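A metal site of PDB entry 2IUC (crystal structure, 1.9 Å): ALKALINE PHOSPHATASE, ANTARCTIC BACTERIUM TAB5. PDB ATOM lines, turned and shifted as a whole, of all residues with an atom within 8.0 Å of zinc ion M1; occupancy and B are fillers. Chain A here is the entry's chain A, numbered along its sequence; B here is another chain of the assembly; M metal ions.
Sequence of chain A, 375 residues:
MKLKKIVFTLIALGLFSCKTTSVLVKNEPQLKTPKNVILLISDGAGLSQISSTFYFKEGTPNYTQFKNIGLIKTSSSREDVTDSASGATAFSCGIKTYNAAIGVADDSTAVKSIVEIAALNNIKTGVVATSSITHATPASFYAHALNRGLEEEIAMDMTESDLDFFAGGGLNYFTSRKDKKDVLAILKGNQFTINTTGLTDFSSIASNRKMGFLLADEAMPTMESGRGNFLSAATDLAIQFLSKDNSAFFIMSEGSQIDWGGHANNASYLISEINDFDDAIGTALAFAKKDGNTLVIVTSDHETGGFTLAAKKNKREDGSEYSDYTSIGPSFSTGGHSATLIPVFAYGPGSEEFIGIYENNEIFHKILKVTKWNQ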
ATOM      1  N   ASP A  43     -17.368 -14.273 -20.766  1.00  0.00           N
ATOM      2  CA  ASP A  43     -18.258 -14.824 -21.756  1.00  0.00           C
ATOM      3  C   ASP A  43     -17.795 -14.603 -23.154  1.00  0.00           C
ATOM      4  O   ASP A  43     -17.621 -13.452 -23.574  1.00  0.00           O
ATOM      5  CB  ASP A  43     -19.655 -14.228 -21.610  1.00  0.00           C
ATOM      6  CG  ASP A  43     -20.746 -15.126 -22.278  1.00  0.00           C
ATOM      7  OD1 ASP A  43     -20.637 -15.456 -23.435  1.00  0.00           O
ATOM      8  OD2 ASP A  43     -21.714 -15.516 -21.608  1.00  0.00           O
ATOM      9  N   GLY A  44     -17.600 -15.697 -23.902  1.00  0.00           N
ATOM     10  CA  GLY A  44     -17.228 -15.549 -25.304  1.00  0.00           C
ATOM     11  C   GLY A  44     -15.774 -15.270 -25.627  1.00  0.00           C
ATOM     12  O   GLY A  44     -15.481 -14.927 -26.753  1.00  0.00           O
ATOM     13  N   THR A  82     -21.743 -24.766 -28.219  1.00  0.00           N
ATOM     14  CA  THR A  82     -22.548 -24.545 -27.050  1.00  0.00           C
ATOM     15  C   THR A  82     -23.109 -23.113 -27.074  1.00  0.00           C
ATOM     16  O   THR A  82     -22.576 -22.256 -27.774  1.00  0.00           O
ATOM     17  CB  THR A  82     -21.669 -24.696 -25.763  1.00  0.00           C
ATOM     18  OG1 THR A  82     -22.539 -24.716 -24.618  1.00  0.00           O
ATOM     19  CG2 THR A  82     -20.755 -23.495 -25.634  1.00  0.00           C
ATOM     20  N   ASP A  83     -24.149 -22.868 -26.314  1.00  0.00           N
ATOM     21  CA  ASP A  83     -24.512 -21.466 -25.961  1.00  0.00           C
ATOM     22  C   ASP A  83     -24.092 -21.199 -24.515  1.00  0.00           C
ATOM     23  O   ASP A  83     -23.557 -22.087 -23.821  1.00  0.00           O
ATOM     24  CB  ASP A  83     -26.043 -21.194 -26.226  1.00  0.00           C
ATOM     25  CG  ASP A  83     -26.965 -21.680 -25.100  1.00  0.00           C
ATOM     26  OD1 ASP A  83     -26.692 -22.670 -24.346  1.00  0.00           O
ATOM     27  OD2 ASP A  83     -28.043 -21.076 -24.972  1.00  0.00           O
ATOM     28  N   SER A  84     -24.385 -20.003 -24.025  1.00  0.00           N
ATOM     29  CA  SER A  84     -23.947 -19.660 -22.659  1.00  0.00           C
ATOM     30  C   SER A  84     -24.674 -20.436 -21.573  1.00  0.00           C
ATOM     31  O   SER A  84     -24.183 -20.603 -20.419  1.00  0.00           O
ATOM     32  CB  SER A  84     -24.343 -18.220 -22.428  1.00  0.00           C
ATOM     33  OG  SER A  84     -23.565 -17.459 -23.291  1.00  0.00           O
ATOM     34  N   HIS A 135     -29.443 -12.938 -16.943  1.00  0.00           N
ATOM     35  CA  HIS A 135     -28.824 -13.463 -18.201  1.00  0.00           C
ATOM     36  C   HIS A 135     -28.260 -14.899 -17.964  1.00  0.00           C
ATOM     37  O   HIS A 135     -28.125 -15.284 -16.837  1.00  0.00           O
ATOM     38  CB  HIS A 135     -27.715 -12.525 -18.753  1.00  0.00           C
ATOM     39  CG  HIS A 135     -27.633 -12.538 -20.256  1.00  0.00           C
ATOM     40  ND1 HIS A 135     -26.660 -13.244 -20.940  1.00  0.00           N
ATOM     41  CD2 HIS A 135     -28.431 -11.962 -21.210  1.00  0.00           C
ATOM     42  CE1 HIS A 135     -26.871 -13.104 -22.247  1.00  0.00           C
ATOM     43  NE2 HIS A 135     -27.932 -12.324 -22.432  1.00  0.00           N
ATOM     44  N   ARG A 148     -33.471 -20.481 -21.131  1.00  0.00           N
ATOM     45  CA  ARG A 148     -32.811 -19.270 -20.661  1.00  0.00           C
ATOM     46  C   ARG A 148     -33.623 -18.031 -20.963  1.00  0.00           C
ATOM     47  O   ARG A 148     -33.340 -17.006 -20.393  1.00  0.00           O
ATOM     48  CB  ARG A 148     -31.486 -19.081 -21.436  1.00  0.00           C
ATOM     49  CG  ARG A 148     -31.683 -18.991 -22.986  1.00  0.00           C
ATOM     50  CD  ARG A 148     -30.338 -18.966 -23.572  1.00  0.00           C
ATOM     51  NE  ARG A 148     -29.649 -17.694 -23.284  1.00  0.00           N
ATOM     52  CZ  ARG A 148     -28.438 -17.363 -23.749  1.00  0.00           C
ATOM     53  NH1 ARG A 148     -27.729 -18.284 -24.476  1.00  0.00           N
ATOM     54  NH2 ARG A 148     -27.917 -16.152 -23.471  1.00  0.00           N
ATOM     55  N   SER A 256     -19.512 -10.206 -18.884  1.00  0.00           N
ATOM     56  CA  SER A 256     -20.655 -10.615 -19.755  1.00  0.00           C
ATOM     57  C   SER A 256     -20.631 -10.105 -21.165  1.00  0.00           C
ATOM     58  O   SER A 256     -21.154 -10.791 -22.099  1.00  0.00           O
ATOM     59  CB  SER A 256     -21.999 -10.167 -19.137  1.00  0.00           C
ATOM     60  OG  SER A 256     -22.005 -10.410 -17.760  1.00  0.00           O
ATOM     61  N   ILE A 258     -18.169  -9.195 -23.203  1.00  0.00           N
ATOM     62  CA  ILE A 258     -17.155  -9.615 -24.199  1.00  0.00           C
ATOM     63  C   ILE A 258     -17.826 -10.345 -25.400  1.00  0.00           C
ATOM     64  O   ILE A 258     -17.466 -10.174 -26.592  1.00  0.00           O
ATOM     65  CB  ILE A 258     -16.137 -10.545 -23.552  1.00  0.00           C
ATOM     66  CG1 ILE A 258     -15.373  -9.757 -22.468  1.00  0.00           C
ATOM     67  CG2 ILE A 258     -15.076 -10.959 -24.587  1.00  0.00           C
ATOM     68  CD1 ILE A 258     -14.664 -10.645 -21.421  1.00  0.00           C
ATOM     69  N   ASP A 259     -18.716 -11.235 -25.066  1.00  0.00           N
ATOM     70  CA  ASP A 259     -19.431 -12.028 -26.098  1.00  0.00           C
ATOM     71  C   ASP A 259     -20.271 -11.096 -26.998  1.00  0.00           C
ATOM     72  O   ASP A 259     -20.484 -11.322 -28.198  1.00  0.00           O
ATOM     73  CB  ASP A 259     -20.341 -12.957 -25.315  1.00  0.00           C
ATOM     74  CG  ASP A 259     -21.359 -13.673 -26.222  1.00  0.00           C
ATOM     75  OD1 ASP A 259     -20.959 -14.647 -26.873  1.00  0.00           O
ATOM     76  OD2 ASP A 259     -22.545 -13.265 -26.231  1.00  0.00           O
ATOM     77  N   TRP A 260     -20.777 -10.014 -26.426  1.00  0.00           N
ATOM     78  CA  TRP A 260     -21.684  -9.170 -27.250  1.00  0.00           C
ATOM     79  C   TRP A 260     -20.901  -8.419 -28.272  1.00  0.00           C
ATOM     80  O   TRP A 260     -21.392  -8.177 -29.362  1.00  0.00           O
ATOM     81  CB  TRP A 260     -22.547  -8.232 -26.377  1.00  0.00           C
ATOM     82  CG  TRP A 260     -23.378  -8.972 -25.284  1.00  0.00           C
ATOM     83  CD1 TRP A 260     -23.543 -10.358 -25.131  1.00  0.00           C
ATOM     84  CD2 TRP A 260     -24.152  -8.365 -24.245  1.00  0.00           C
ATOM     85  NE1 TRP A 260     -24.367 -10.616 -24.064  1.00  0.00           N
ATOM     86  CE2 TRP A 260     -24.774  -9.405 -23.504  1.00  0.00           C
ATOM     87  CE3 TRP A 260     -24.426  -7.024 -23.894  1.00  0.00           C
ATOM     88  CZ2 TRP A 260     -25.601  -9.149 -22.408  1.00  0.00           C
ATOM     89  CZ3 TRP A 260     -25.235  -6.752 -22.805  1.00  0.00           C
ATOM     90  CH2 TRP A 260     -25.845  -7.796 -22.094  1.00  0.00           C
ATOM     91  N   GLY A 262     -18.208  -9.776 -29.626  1.00  0.00           N
ATOM     92  CA  GLY A 262     -17.893 -10.788 -30.636  1.00  0.00           C
ATOM     93  C   GLY A 262     -19.091 -10.920 -31.596  1.00  0.00           C
ATOM     94  O   GLY A 262     -18.871 -10.918 -32.783  1.00  0.00           O
ATOM     95  N   HIS A 263     -20.316 -11.010 -31.092  1.00  0.00           N
ATOM     96  CA  HIS A 263     -21.523 -11.159 -31.931  1.00  0.00           C
ATOM     97  C   HIS A 263     -21.677  -9.957 -32.827  1.00  0.00           C
ATOM     98  O   HIS A 263     -22.150 -10.112 -33.936  1.00  0.00           O
ATOM     99  CB  HIS A 263     -22.810 -11.242 -31.092  1.00  0.00           C
ATOM    100  CG  HIS A 263     -23.065 -12.591 -30.483  1.00  0.00           C
ATOM    101  ND1 HIS A 263     -23.174 -13.759 -31.235  1.00  0.00           N
ATOM    102  CD2 HIS A 263     -23.297 -12.951 -29.194  1.00  0.00           C
ATOM    103  CE1 HIS A 263     -23.430 -14.780 -30.429  1.00  0.00           C
ATOM    104  NE2 HIS A 263     -23.523 -14.312 -29.189  1.00  0.00           N
ATOM    105  N   ASP A 301     -17.006 -19.529 -21.222  1.00  0.00           N
ATOM    106  CA  ASP A 301     -17.924 -20.578 -21.665  1.00  0.00           C
ATOM    107  C   ASP A 301     -17.704 -21.139 -23.085  1.00  0.00           C
ATOM    108  O   ASP A 301     -18.037 -22.307 -23.343  1.00  0.00           O
ATOM    109  CB  ASP A 301     -19.388 -20.161 -21.458  1.00  0.00           C
ATOM    110  CG  ASP A 301     -19.744 -18.780 -22.101  1.00  0.00           C
ATOM    111  OD1 ASP A 301     -18.899 -18.048 -22.682  1.00  0.00           O
ATOM    112  OD2 ASP A 301     -20.958 -18.478 -22.153  1.00  0.00           O
ATOM    113  N   HIS A 302     -17.194 -20.321 -24.015  1.00  0.00           N
ATOM    114  CA  HIS A 302     -16.980 -20.686 -25.430  1.00  0.00           C
ATOM    115  C   HIS A 302     -16.390 -19.382 -26.021  1.00  0.00           C
ATOM    116  O   HIS A 302     -16.306 -18.338 -25.328  1.00  0.00           O
ATOM    117  CB  HIS A 302     -18.354 -21.027 -26.135  1.00  0.00           C
ATOM    118  CG  HIS A 302     -19.334 -19.883 -25.993  1.00  0.00           C
ATOM    119  ND1 HIS A 302     -19.202 -18.717 -26.708  1.00  0.00           N
ATOM    120  CD2 HIS A 302     -20.337 -19.664 -25.118  1.00  0.00           C
ATOM    121  CE1 HIS A 302     -20.051 -17.826 -26.276  1.00  0.00           C
ATOM    122  NE2 HIS A 302     -20.775 -18.375 -25.340  1.00  0.00           N
ATOM    123  N   GLU A 303     -15.960 -19.455 -27.287  1.00  0.00           N
ATOM    124  CA  GLU A 303     -15.450 -18.355 -28.061  1.00  0.00           C
ATOM    125  C   GLU A 303     -16.575 -17.757 -28.915  1.00  0.00           C
ATOM    126  O   GLU A 303     -17.493 -18.480 -29.319  1.00  0.00           O
ATOM    127  CB  GLU A 303     -14.412 -18.917 -29.030  1.00  0.00           C
ATOM    128  CG  GLU A 303     -13.572 -17.829 -29.647  1.00  0.00           C
ATOM    129  CD  GLU A 303     -14.088 -17.228 -31.013  1.00  0.00           C
ATOM    130  OE1 GLU A 303     -14.997 -17.810 -31.697  1.00  0.00           O
ATOM    131  OE2 GLU A 303     -13.478 -16.210 -31.427  1.00  0.00           O
ATOM    132  N   THR A 304     -16.485 -16.467 -29.198  1.00  0.00           N
ATOM    133  CA  THR A 304     -17.445 -15.858 -30.154  1.00  0.00           C
ATOM    134  C   THR A 304     -16.844 -14.965 -31.265  1.00  0.00           C
ATOM    135  O   THR A 304     -15.992 -14.063 -31.015  1.00  0.00           O
ATOM    136  CB  THR A 304     -18.418 -14.931 -29.413  1.00  0.00           C
ATOM    137  OG1 THR A 304     -18.999 -15.628 -28.342  1.00  0.00           O
ATOM    138  CG2 THR A 304     -19.605 -14.423 -30.412  1.00  0.00           C
ATOM    139  N   GLY A 305     -17.375 -15.130 -32.490  1.00  0.00           N
ATOM    140  CA  GLY A 305     -16.955 -14.270 -33.600  1.00  0.00           C
ATOM    141  C   GLY A 305     -15.774 -14.705 -34.479  1.00  0.00           C
ATOM    142  O   GLY A 305     -15.537 -14.055 -35.511  1.00  0.00           O
ATOM    143  N   GLY A 335     -20.724 -14.490 -36.738  1.00  0.00           N
ATOM    144  CA  GLY A 335     -21.518 -13.620 -35.857  1.00  0.00           C
ATOM    145  C   GLY A 335     -21.955 -14.450 -34.685  1.00  0.00           C
ATOM    146  O   GLY A 335     -22.642 -13.947 -33.808  1.00  0.00           O
ATOM    147  N   GLY A 336     -21.629 -15.747 -34.702  1.00  0.00           N
ATOM    148  CA  GLY A 336     -21.998 -16.703 -33.636  1.00  0.00           C
ATOM    149  C   GLY A 336     -20.830 -17.246 -32.810  1.00  0.00           C
ATOM    150  O   GLY A 336     -19.710 -16.733 -32.919  1.00  0.00           O
ATOM    151  N   HIS A 337     -21.103 -18.291 -32.012  1.00  0.00           N
ATOM    152  CA  HIS A 337     -20.133 -18.954 -31.105  1.00  0.00           C
ATOM    153  C   HIS A 337     -19.276 -19.887 -31.942  1.00  0.00           C
ATOM    154  O   HIS A 337     -19.600 -20.185 -33.109  1.00  0.00           O
ATOM    155  CB  HIS A 337     -20.909 -19.741 -30.023  1.00  0.00           C
ATOM    156  CG  HIS A 337     -21.715 -18.869 -29.098  1.00  0.00           C
ATOM    157  ND1 HIS A 337     -22.569 -19.389 -28.153  1.00  0.00           N
ATOM    158  CD2 HIS A 337     -21.849 -17.501 -29.022  1.00  0.00           C
ATOM    159  CE1 HIS A 337     -23.189 -18.384 -27.513  1.00  0.00           C
ATOM    160  NE2 HIS A 337     -22.709 -17.247 -27.980  1.00  0.00           N
ATOM    161  N   TYR B 325     -26.106 -24.913 -34.574  1.00  0.00           N
ATOM    162  CA  TYR B 325     -25.055 -25.173 -33.579  1.00  0.00           C
ATOM    163  C   TYR B 325     -24.809 -26.654 -33.349  1.00  0.00           C
ATOM    164  O   TYR B 325     -23.821 -27.056 -32.676  1.00  0.00           O
ATOM    165  CB  TYR B 325     -25.430 -24.493 -32.260  1.00  0.00           C
ATOM    166  CG  TYR B 325     -25.050 -22.998 -32.204  1.00  0.00           C
ATOM    167  CD1 TYR B 325     -25.033 -22.210 -33.358  1.00  0.00           C
ATOM    168  CD2 TYR B 325     -24.713 -22.391 -30.994  1.00  0.00           C
ATOM    169  CE1 TYR B 325     -24.701 -20.818 -33.321  1.00  0.00           C
ATOM    170  CE2 TYR B 325     -24.405 -21.008 -30.927  1.00  0.00           C
ATOM    171  CZ  TYR B 325     -24.381 -20.249 -32.084  1.00  0.00           C
ATOM    172  OH  TYR B 325     -24.035 -18.931 -32.006  1.00  0.00           O
HETATM  173 ZN    ZN M   1     -23.123 -15.329 -27.372  1.00  0.00          ZN
HETATM  174 ZN    ZN M   2     -21.604 -17.250 -23.731  1.00  0.00          ZN
HETATM  175 MG    MG M   3     -23.002 -14.603 -20.279  1.00  0.00          MG
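Zinc ion M1 is bound by NE2 of His 337 (2.1 Å), NE2 of His 263 (2.1 Å), OD1 of Asp 259 (2.3 Å) and OD2 of Asp 259 (2.4 Å).
Three residues have an atom within 4 Å of zinc ion M1: Asp 259, His 263 and His 337.
A ring nitrogen (NE2) of His 302 lies close to a ring nitrogen (ND1) of His 337, at 3.5 Å.
N of His 337 lies within hydrogen-bond range of OH of Tyr 325 of chain B (3.0 Å).
A ring nitrogen (ND1) of His 337 is in hydrogen-bond range of the backbone carbonyl oxygen (O) of Thr 82.
A ring nitrogen (ND1) of His 263 sits at hydrogen-bond distance from the backbone carbonyl oxygen (O) of Gly 335 (2.6 Å).
The side-chain carboxylate (OD1) of Asp 259 lies close to the side-chain hydroxyl (OG1) of Thr 304 (2.6 Å).
The backbone NH (N) of Asp 259 sits at hydrogen-bond distance from the backbone carbonyl oxygen (O) of Asp 43, at 2.9 Å.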
